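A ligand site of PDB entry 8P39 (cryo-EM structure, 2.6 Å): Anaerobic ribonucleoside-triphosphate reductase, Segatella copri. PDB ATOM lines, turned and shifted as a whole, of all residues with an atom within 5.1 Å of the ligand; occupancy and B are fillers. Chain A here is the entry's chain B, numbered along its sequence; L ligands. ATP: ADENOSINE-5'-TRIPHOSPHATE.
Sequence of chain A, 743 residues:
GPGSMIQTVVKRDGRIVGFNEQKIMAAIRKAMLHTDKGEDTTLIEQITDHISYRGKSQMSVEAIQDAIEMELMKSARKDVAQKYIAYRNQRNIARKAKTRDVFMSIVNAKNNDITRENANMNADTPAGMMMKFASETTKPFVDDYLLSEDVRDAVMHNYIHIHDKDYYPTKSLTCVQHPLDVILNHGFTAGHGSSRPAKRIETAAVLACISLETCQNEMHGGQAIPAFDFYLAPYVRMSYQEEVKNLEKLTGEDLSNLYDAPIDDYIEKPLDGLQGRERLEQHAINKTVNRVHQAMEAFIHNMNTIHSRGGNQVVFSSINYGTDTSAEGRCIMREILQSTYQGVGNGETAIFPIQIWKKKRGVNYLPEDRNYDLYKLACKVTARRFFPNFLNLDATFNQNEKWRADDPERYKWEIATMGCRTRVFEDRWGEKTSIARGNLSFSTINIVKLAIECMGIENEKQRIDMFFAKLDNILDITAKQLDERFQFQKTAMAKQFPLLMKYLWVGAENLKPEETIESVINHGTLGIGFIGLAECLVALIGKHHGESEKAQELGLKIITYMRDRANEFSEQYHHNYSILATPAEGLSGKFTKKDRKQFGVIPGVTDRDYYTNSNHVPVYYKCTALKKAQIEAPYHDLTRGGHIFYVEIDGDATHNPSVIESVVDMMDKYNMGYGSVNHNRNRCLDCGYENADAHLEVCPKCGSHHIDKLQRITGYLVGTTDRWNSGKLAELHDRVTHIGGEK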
ATOM      1  N   GLU A 117      10.831  -6.344  13.412  1.00  0.00           N
ATOM      2  CA  GLU A 117      11.764  -5.228  13.524  1.00  0.00           C
ATOM      3  C   GLU A 117      13.162  -5.700  13.888  1.00  0.00           C
ATOM      4  O   GLU A 117      14.159  -5.154  13.406  1.00  0.00           O
ATOM      5  CB  GLU A 117      11.258  -4.229  14.564  1.00  0.00           C
ATOM      6  CG  GLU A 117      12.177  -3.045  14.779  1.00  0.00           C
ATOM      7  CD  GLU A 117      11.784  -2.212  15.983  1.00  0.00           C
ATOM      8  OE1 GLU A 117      10.995  -2.713  16.811  1.00  0.00           O
ATOM      9  OE2 GLU A 117      12.268  -1.065  16.101  1.00  0.00           O
ATOM     10  N   ASN A 118      13.269  -6.718  14.746  1.00  0.00           N
ATOM     11  CA  ASN A 118      14.534  -7.195  15.271  1.00  0.00           C
ATOM     12  C   ASN A 118      14.703  -8.678  14.945  1.00  0.00           C
ATOM     13  O   ASN A 118      13.758  -9.460  15.088  1.00  0.00           O
ATOM     14  CB  ASN A 118      14.610  -6.977  16.784  1.00  0.00           C
ATOM     15  CG  ASN A 118      16.021  -6.970  17.313  1.00  0.00           C
ATOM     16  OD1 ASN A 118      16.909  -7.636  16.757  1.00  0.00           O
ATOM     17  ND2 ASN A 118      16.251  -6.232  18.387  1.00  0.00           N
ATOM     18  N   ASN A 120      17.125 -10.744  16.331  1.00  0.00           N
ATOM     19  CA  ASN A 120      17.559 -11.545  17.463  1.00  0.00           C
ATOM     20  C   ASN A 120      16.414 -12.095  18.291  1.00  0.00           C
ATOM     21  O   ASN A 120      16.643 -12.956  19.143  1.00  0.00           O
ATOM     22  CB  ASN A 120      18.490 -10.727  18.366  1.00  0.00           C
ATOM     23  CG  ASN A 120      19.804 -10.387  17.698  1.00  0.00           C
ATOM     24  OD1 ASN A 120      20.735 -11.195  17.689  1.00  0.00           O
ATOM     25  ND2 ASN A 120      19.890  -9.186  17.149  1.00  0.00           N
ATOM     26  N   HIS A 161      15.379  10.435  14.059  1.00  0.00           N
ATOM     27  CA  HIS A 161      14.983   9.110  14.510  1.00  0.00           C
ATOM     28  C   HIS A 161      15.728   8.776  15.790  1.00  0.00           C
ATOM     29  O   HIS A 161      16.928   9.055  15.923  1.00  0.00           O
ATOM     30  CB  HIS A 161      15.286   8.044  13.454  1.00  0.00           C
ATOM     31  CG  HIS A 161      14.949   6.658  13.887  1.00  0.00           C
ATOM     32  ND1 HIS A 161      13.694   6.103  13.716  1.00  0.00           N
ATOM     33  CD2 HIS A 161      15.706   5.701  14.475  1.00  0.00           C
ATOM     34  CE1 HIS A 161      13.695   4.866  14.185  1.00  0.00           C
ATOM     35  NE2 HIS A 161      14.902   4.597  14.650  1.00  0.00           N
ATOM     36  N   ILE A 162      15.015   8.184  16.738  1.00  0.00           N
ATOM     37  CA  ILE A 162      15.585   7.771  18.014  1.00  0.00           C
ATOM     38  C   ILE A 162      15.766   6.253  17.998  1.00  0.00           C
ATOM     39  O   ILE A 162      14.960   5.529  17.399  1.00  0.00           O
ATOM     40  CB  ILE A 162      14.691   8.213  19.193  1.00  0.00           C
ATOM     41  CG1 ILE A 162      14.267   9.669  19.003  1.00  0.00           C
ATOM     42  CG2 ILE A 162      15.421   8.031  20.507  1.00  0.00           C
ATOM     43  CD1 ILE A 162      13.300  10.156  20.057  1.00  0.00           C
ATOM     44  N   HIS A 163      16.829   5.782  18.625  1.00  0.00           N
ATOM     45  CA  HIS A 163      17.156   4.364  18.652  1.00  0.00           C
ATOM     46  C   HIS A 163      16.779   3.762  20.000  1.00  0.00           C
ATOM     47  O   HIS A 163      17.101   4.333  21.043  1.00  0.00           O
ATOM     48  CB  HIS A 163      18.643   4.134  18.366  1.00  0.00           C
ATOM     49  CG  HIS A 163      19.042   4.456  16.962  1.00  0.00           C
ATOM     50  ND1 HIS A 163      18.737   3.641  15.903  1.00  0.00           N
ATOM     51  CD2 HIS A 163      19.719   5.506  16.452  1.00  0.00           C
ATOM     52  CE1 HIS A 163      19.214   4.172  14.784  1.00  0.00           C
ATOM     53  NE2 HIS A 163      19.809   5.305  15.095  1.00  0.00           N
ATOM     54  N   ASP A 164      16.074   2.627  19.961  1.00  0.00           N
ATOM     55  CA  ASP A 164      15.618   1.924  21.154  1.00  0.00           C
ATOM     56  C   ASP A 164      14.691   2.811  21.988  1.00  0.00           C
ATOM     57  O   ASP A 164      14.948   3.124  23.149  1.00  0.00           O
ATOM     58  CB  ASP A 164      16.802   1.421  21.984  1.00  0.00           C
ATOM     59  CG  ASP A 164      17.692   0.463  21.198  1.00  0.00           C
ATOM     60  OD1 ASP A 164      17.146  -0.410  20.490  1.00  0.00           O
ATOM     61  OD2 ASP A 164      18.928   0.582  21.294  1.00  0.00           O
ATOM     62  N   GLN A 216      23.353  -8.799  30.724  1.00  0.00           N
ATOM     63  CA  GLN A 216      22.498  -8.514  29.575  1.00  0.00           C
ATOM     64  C   GLN A 216      21.123  -8.057  30.021  1.00  0.00           C
ATOM     65  O   GLN A 216      20.546  -7.130  29.428  1.00  0.00           O
ATOM     66  CB  GLN A 216      22.383  -9.741  28.680  1.00  0.00           C
ATOM     67  CG  GLN A 216      21.464  -9.546  27.498  1.00  0.00           C
ATOM     68  CD  GLN A 216      21.956  -8.482  26.543  1.00  0.00           C
ATOM     69  OE1 GLN A 216      22.723  -8.770  25.626  1.00  0.00           O
ATOM     70  NE2 GLN A 216      21.520  -7.242  26.739  1.00  0.00           N
ATOM     71  N   HIS A 220      20.247  -2.755  27.126  1.00  0.00           N
ATOM     72  CA  HIS A 220      19.562  -3.047  25.874  1.00  0.00           C
ATOM     73  C   HIS A 220      20.519  -3.226  24.699  1.00  0.00           C
ATOM     74  O   HIS A 220      20.079  -3.212  23.550  1.00  0.00           O
ATOM     75  CB  HIS A 220      18.548  -1.953  25.554  1.00  0.00           C
ATOM     76  CG  HIS A 220      19.154  -0.620  25.258  1.00  0.00           C
ATOM     77  ND1 HIS A 220      19.092   0.441  26.137  1.00  0.00           N
ATOM     78  CD2 HIS A 220      19.834  -0.164  24.175  1.00  0.00           C
ATOM     79  CE1 HIS A 220      19.706   1.487  25.605  1.00  0.00           C
ATOM     80  NE2 HIS A 220      20.160   1.150  24.422  1.00  0.00           N
ATOM     81  N   GLY A 221      21.822  -3.398  24.958  1.00  0.00           N
ATOM     82  CA  GLY A 221      22.805  -3.515  23.912  1.00  0.00           C
ATOM     83  C   GLY A 221      23.679  -4.753  24.100  1.00  0.00           C
ATOM     84  O   GLY A 221      23.256  -5.760  24.661  1.00  0.00           O
ATOM     85  N   GLY A 222      24.927  -4.639  23.619  1.00  0.00           N
ATOM     86  CA  GLY A 222      25.834  -5.759  23.613  1.00  0.00           C
ATOM     87  C   GLY A 222      26.750  -5.819  24.824  1.00  0.00           C
ATOM     88  O   GLY A 222      26.773  -4.919  25.672  1.00  0.00           O
ATOM     89  N   GLN A 313      15.820  -9.588  27.458  1.00  0.00           N
ATOM     90  CA  GLN A 313      16.526  -9.121  26.271  1.00  0.00           C
ATOM     91  C   GLN A 313      17.558 -10.153  25.835  1.00  0.00           C
ATOM     92  O   GLN A 313      18.258 -10.740  26.657  1.00  0.00           O
ATOM     93  CB  GLN A 313      17.196  -7.768  26.546  1.00  0.00           C
ATOM     94  CG  GLN A 313      17.703  -7.057  25.309  1.00  0.00           C
ATOM     95  CD  GLN A 313      16.585  -6.453  24.476  1.00  0.00           C
ATOM     96  OE1 GLN A 313      15.424  -6.434  24.891  1.00  0.00           O
ATOM     97  NE2 GLN A 313      16.921  -5.952  23.298  1.00  0.00           N
ATOM     98  N   VAL A 314      17.642 -10.370  24.521  1.00  0.00           N
ATOM     99  CA  VAL A 314      18.525 -11.399  23.988  1.00  0.00           C
ATOM    100  C   VAL A 314      19.980 -11.038  24.279  1.00  0.00           C
ATOM    101  O   VAL A 314      20.356  -9.860  24.353  1.00  0.00           O
ATOM    102  CB  VAL A 314      18.282 -11.570  22.473  1.00  0.00           C
ATOM    103  CG1 VAL A 314      18.829 -12.907  22.003  1.00  0.00           C
ATOM    104  CG2 VAL A 314      16.802 -11.456  22.165  1.00  0.00           C
ATOM    105  N   PHE A 316      23.806 -10.464  23.842  1.00  0.00           N
ATOM    106  CA  PHE A 316      24.725  -9.999  22.818  1.00  0.00           C
ATOM    107  C   PHE A 316      26.115  -9.918  23.435  1.00  0.00           C
ATOM    108  O   PHE A 316      26.349  -9.112  24.342  1.00  0.00           O
ATOM    109  CB  PHE A 316      24.289  -8.632  22.281  1.00  0.00           C
ATOM    110  CG  PHE A 316      24.780  -8.336  20.896  1.00  0.00           C
ATOM    111  CD1 PHE A 316      26.084  -7.931  20.674  1.00  0.00           C
ATOM    112  CD2 PHE A 316      23.923  -8.435  19.814  1.00  0.00           C
ATOM    113  CE1 PHE A 316      26.532  -7.653  19.391  1.00  0.00           C
ATOM    114  CE2 PHE A 316      24.363  -8.151  18.530  1.00  0.00           C
ATOM    115  CZ  PHE A 316      25.665  -7.763  18.322  1.00  0.00           C
ATOM    116  N   GLY A 419      30.211  -5.038  20.707  1.00  0.00           N
ATOM    117  CA  GLY A 419      29.346  -5.569  19.664  1.00  0.00           C
ATOM    118  C   GLY A 419      29.022  -4.527  18.613  1.00  0.00           C
ATOM    119  O   GLY A 419      29.114  -3.319  18.850  1.00  0.00           O
ATOM    120  N   CYS A 420      28.635  -5.025  17.445  1.00  0.00           N
ATOM    121  CA  CYS A 420      28.335  -4.190  16.277  1.00  0.00           C
ATOM    122  C   CYS A 420      29.576  -3.439  15.817  1.00  0.00           C
ATOM    123  O   CYS A 420      30.517  -4.042  15.308  1.00  0.00           O
ATOM    124  CB  CYS A 420      27.187  -3.223  16.573  1.00  0.00           C
ATOM    125  SG  CYS A 420      26.831  -2.087  15.228  1.00  0.00           S
ATOM    126  N   PHE A 442      22.249   7.089  21.042  1.00  0.00           N
ATOM    127  CA  PHE A 442      22.599   7.648  19.742  1.00  0.00           C
ATOM    128  C   PHE A 442      21.346   7.777  18.891  1.00  0.00           C
ATOM    129  O   PHE A 442      20.393   7.002  19.033  1.00  0.00           O
ATOM    130  CB  PHE A 442      23.664   6.801  19.031  1.00  0.00           C
ATOM    131  CG  PHE A 442      23.275   5.363  18.831  1.00  0.00           C
ATOM    132  CD1 PHE A 442      23.319   4.472  19.890  1.00  0.00           C
ATOM    133  CD2 PHE A 442      22.904   4.902  17.584  1.00  0.00           C
ATOM    134  CE1 PHE A 442      22.973   3.143  19.705  1.00  0.00           C
ATOM    135  CE2 PHE A 442      22.563   3.579  17.393  1.00  0.00           C
ATOM    136  CZ  PHE A 442      22.603   2.699  18.457  1.00  0.00           C
ATOM    137  N   THR A 582      25.917   4.925  11.360  1.00  0.00           N
ATOM    138  CA  THR A 582      24.798   4.233  11.976  1.00  0.00           C
ATOM    139  C   THR A 582      24.492   2.939  11.238  1.00  0.00           C
ATOM    140  O   THR A 582      24.387   2.941  10.012  1.00  0.00           O
ATOM    141  CB  THR A 582      23.564   5.130  12.000  1.00  0.00           C
ATOM    142  OG1 THR A 582      23.835   6.316  12.759  1.00  0.00           O
ATOM    143  CG2 THR A 582      22.377   4.400  12.623  1.00  0.00           C
ATOM    144  N   PRO A 583      24.359   1.809  11.942  1.00  0.00           N
ATOM    145  CA  PRO A 583      23.926   0.581  11.278  1.00  0.00           C
ATOM    146  C   PRO A 583      22.503   0.707  10.756  1.00  0.00           C
ATOM    147  O   PRO A 583      21.674   1.435  11.317  1.00  0.00           O
ATOM    148  CB  PRO A 583      24.015  -0.472  12.393  1.00  0.00           C
ATOM    149  CG  PRO A 583      24.878   0.140  13.439  1.00  0.00           C
ATOM    150  CD  PRO A 583      24.637   1.611  13.371  1.00  0.00           C
ATOM    151  N   ALA A 584      22.230  -0.006   9.668  1.00  0.00           N
ATOM    152  CA  ALA A 584      20.929   0.051   9.007  1.00  0.00           C
ATOM    153  C   ALA A 584      20.275  -1.323   9.085  1.00  0.00           C
ATOM    154  O   ALA A 584      20.509  -2.187   8.240  1.00  0.00           O
ATOM    155  CB  ALA A 584      21.085   0.508   7.551  1.00  0.00           C
ATOM    156  N   GLU A 585      19.454  -1.526  10.124  1.00  0.00           N
ATOM    157  CA  GLU A 585      18.658  -2.742  10.262  1.00  0.00           C
ATOM    158  C   GLU A 585      17.166  -2.473  10.216  1.00  0.00           C
ATOM    159  O   GLU A 585      16.454  -3.098   9.426  1.00  0.00           O
ATOM    160  CB  GLU A 585      19.013  -3.457  11.581  1.00  0.00           C
ATOM    161  CG  GLU A 585      18.171  -4.689  11.849  1.00  0.00           C
ATOM    162  CD  GLU A 585      18.160  -5.088  13.314  1.00  0.00           C
ATOM    163  OE1 GLU A 585      18.909  -4.481  14.103  1.00  0.00           O
ATOM    164  OE2 GLU A 585      17.397  -6.002  13.671  1.00  0.00           O
ATOM    165  N   GLY A 586      16.662  -1.552  11.032  1.00  0.00           N
ATOM    166  CA  GLY A 586      15.259  -1.210  11.023  1.00  0.00           C
ATOM    167  C   GLY A 586      15.001   0.166  10.451  1.00  0.00           C
ATOM    168  O   GLY A 586      13.950   0.412   9.849  1.00  0.00           O
ATOM    169  N   LEU A 587      15.953   1.076  10.639  1.00  0.00           N
ATOM    170  CA  LEU A 587      15.865   2.404  10.040  1.00  0.00           C
ATOM    171  C   LEU A 587      16.115   2.381   8.546  1.00  0.00           C
ATOM    172  O   LEU A 587      15.872   3.394   7.878  1.00  0.00           O
ATOM    173  CB  LEU A 587      16.840   3.350  10.736  1.00  0.00           C
ATOM    174  CG  LEU A 587      16.622   4.844  10.556  1.00  0.00           C
ATOM    175  CD1 LEU A 587      15.151   5.184  10.717  1.00  0.00           C
ATOM    176  CD2 LEU A 587      17.452   5.618  11.555  1.00  0.00           C
ATOM    177  N   THR A 714      24.049  -5.204   9.440  1.00  0.00           N
ATOM    178  CA  THR A 714      24.955  -4.093   9.691  1.00  0.00           C
ATOM    179  C   THR A 714      25.599  -4.123  11.073  1.00  0.00           C
ATOM    180  O   THR A 714      26.578  -3.404  11.295  1.00  0.00           O
ATOM    181  CB  THR A 714      24.214  -2.768   9.495  1.00  0.00           C
ATOM    182  OG1 THR A 714      23.034  -2.756  10.307  1.00  0.00           O
ATOM    183  CG2 THR A 714      23.816  -2.583   8.037  1.00  0.00           C
ATOM    184  N   GLY A 715      25.086  -4.921  12.014  1.00  0.00           N
ATOM    185  CA  GLY A 715      25.672  -4.957  13.332  1.00  0.00           C
ATOM    186  C   GLY A 715      25.930  -6.327  13.939  1.00  0.00           C
ATOM    187  O   GLY A 715      26.633  -6.427  14.940  1.00  0.00           O
ATOM    188  N   TYR A 716      25.383  -7.391  13.346  1.00  0.00           N
ATOM    189  CA  TYR A 716      25.524  -8.715  13.944  1.00  0.00           C
ATOM    190  C   TYR A 716      25.277  -9.770  12.875  1.00  0.00           C
ATOM    191  O   TYR A 716      25.121  -9.463  11.685  1.00  0.00           O
ATOM    192  CB  TYR A 716      24.581  -8.877  15.144  1.00  0.00           C
ATOM    193  CG  TYR A 716      23.115  -8.649  14.818  1.00  0.00           C
ATOM    194  CD1 TYR A 716      22.316  -9.691  14.392  1.00  0.00           C
ATOM    195  CD2 TYR A 716      22.550  -7.388  14.961  1.00  0.00           C
ATOM    196  CE1 TYR A 716      20.978  -9.490  14.098  1.00  0.00           C
ATOM    197  CE2 TYR A 716      21.215  -7.181  14.675  1.00  0.00           C
ATOM    198  CZ  TYR A 716      20.437  -8.230  14.244  1.00  0.00           C
ATOM    199  OH  TYR A 716      19.107  -8.017  13.950  1.00  0.00           O
HETATM  200  PG  ATP L   1      16.290   0.654  16.616  1.00  0.00           P
HETATM  201  O1G ATP L   1      17.454   1.489  17.027  1.00  0.00           O
HETATM  202  O2G ATP L   1      16.184  -0.676  17.375  1.00  0.00           O
HETATM  203  O3G ATP L   1      14.957   1.384  16.684  1.00  0.00           O
HETATM  204  PB  ATP L   1      17.562   0.018  13.981  1.00  0.00           P
HETATM  205  O1B ATP L   1      17.433  -1.282  13.301  1.00  0.00           O
HETATM  206  O2B ATP L   1      17.540   1.249  13.074  1.00  0.00           O
HETATM  207  O3B ATP L   1      16.439   0.229  15.084  1.00  0.00           O
HETATM  208  PA  ATP L   1      20.443  -0.096  14.610  1.00  0.00           P
HETATM  209  O1A ATP L   1      21.085   1.155  14.173  1.00  0.00           O
HETATM  210  O2A ATP L   1      20.599  -1.268  13.640  1.00  0.00           O
HETATM  211  O3A ATP L   1      18.890   0.089  14.853  1.00  0.00           O
HETATM  212  O5' ATP L   1      20.972  -0.566  16.019  1.00  0.00           O
HETATM  213  C5' ATP L   1      20.814  -1.930  16.473  1.00  0.00           C
HETATM  214  C4' ATP L   1      21.872  -2.223  17.506  1.00  0.00           C
HETATM  215  O4' ATP L   1      21.254  -2.687  18.718  1.00  0.00           O
HETATM  216  C3' ATP L   1      22.858  -3.320  17.117  1.00  0.00           C
HETATM  217  O3' ATP L   1      23.948  -2.794  16.362  1.00  0.00           O
HETATM  218  C2' ATP L   1      23.313  -3.847  18.483  1.00  0.00           C
HETATM  219  O2' ATP L   1      24.360  -3.054  19.023  1.00  0.00           O
HETATM  220  C1' ATP L   1      22.033  -3.714  19.312  1.00  0.00           C
HETATM  221  N9  ATP L   1      21.236  -4.927  19.393  1.00  0.00           N
HETATM  222  C8  ATP L   1      20.646  -5.597  18.349  1.00  0.00           C
HETATM  223  N7  ATP L   1      19.983  -6.676  18.712  1.00  0.00           N
HETATM  224  C5  ATP L   1      20.141  -6.710  20.089  1.00  0.00           C
HETATM  225  C6  ATP L   1      19.680  -7.595  21.076  1.00  0.00           C
HETATM  226  N6  ATP L   1      18.928  -8.672  20.821  1.00  0.00           N
HETATM  227  N1  ATP L   1      20.026  -7.339  22.364  1.00  0.00           N
HETATM  228  C2  ATP L   1      20.773  -6.267  22.626  1.00  0.00           C
HETATM  229  N3  ATP L   1      21.262  -5.367  21.778  1.00  0.00           N
HETATM  230  C4  ATP L   1      20.912  -5.638  20.518  1.00  0.00           C
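N of Gly 586 lies within hydrogen-bond range of O1B of the ligand (2.4 Å). A ring nitrogen (ND1) of His 163 is in hydrogen-bond range of an oxygen (O1G) of the ligand (2.7 Å). The backbone NH (N) of Leu 587 lies within hydrogen-bond range of an oxygen (O2B) of the ligand, at 2.9 Å. An oxygen (O1A) of the ligand lies close to the backbone carbonyl oxygen (O) of Pro 583, at 2.9 Å. N7 of the ligand is in hydrogen-bond range of ND2 of Asn 120 (3.0 Å). SG of Cys 420 is in hydrogen-bond range of O3' of the ligand (3.2 Å). The backbone NH (N) of Asp 164 is in hydrogen-bond range of an oxygen (O1G) of the ligand (3.4 Å).
N of Asn 120 is in hydrogen-bond range of OD1 of Asn 118 (3.1 Å). The side-chain amide nitrogen (ND2) of Asn 120 lies close to the side-chain hydroxyl (OH) of Tyr 716. A ring nitrogen (NE2) of His 220 sits close to the side-chain carboxylate (OD2) of Asp 164, 3.4 Å away. The backbone carbonyl oxygen (O) of Gly 715 lies close to the backbone NH (N) of Cys 420 (3.5 Å). The side-chain hydroxyl (OH) of Tyr 716 is in hydrogen-bond range of the side-chain carboxylate (OE2) of Glu 585 (2.7 Å). The side-chain amide nitrogen (NE2) of Gln 216 is in hydrogen-bond range of the backbone carbonyl oxygen (O) of Gly 221 (3.1 Å). OE1 of Gln 216 lies close to O of Val 314.
A nitrogen (N3) of the ligand lies close to the backbone carbonyl oxygen (O) of His 220 (3.0 Å). N1 of the ligand sits close to O of Val 314, at 3.2 Å. Glu 117 touches the ligand. Asn 118 touches the ligand. NE2 of His 161 touches O3G of the ligand, 3.8 Å away. CA of Gly 221 touches N3 of the ligand (3.2 Å). Gln 313 touches the ligand. Thr 582 touches the ligand. Glu 585 touches the ligand (CB to O1B, 3.2 Å).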
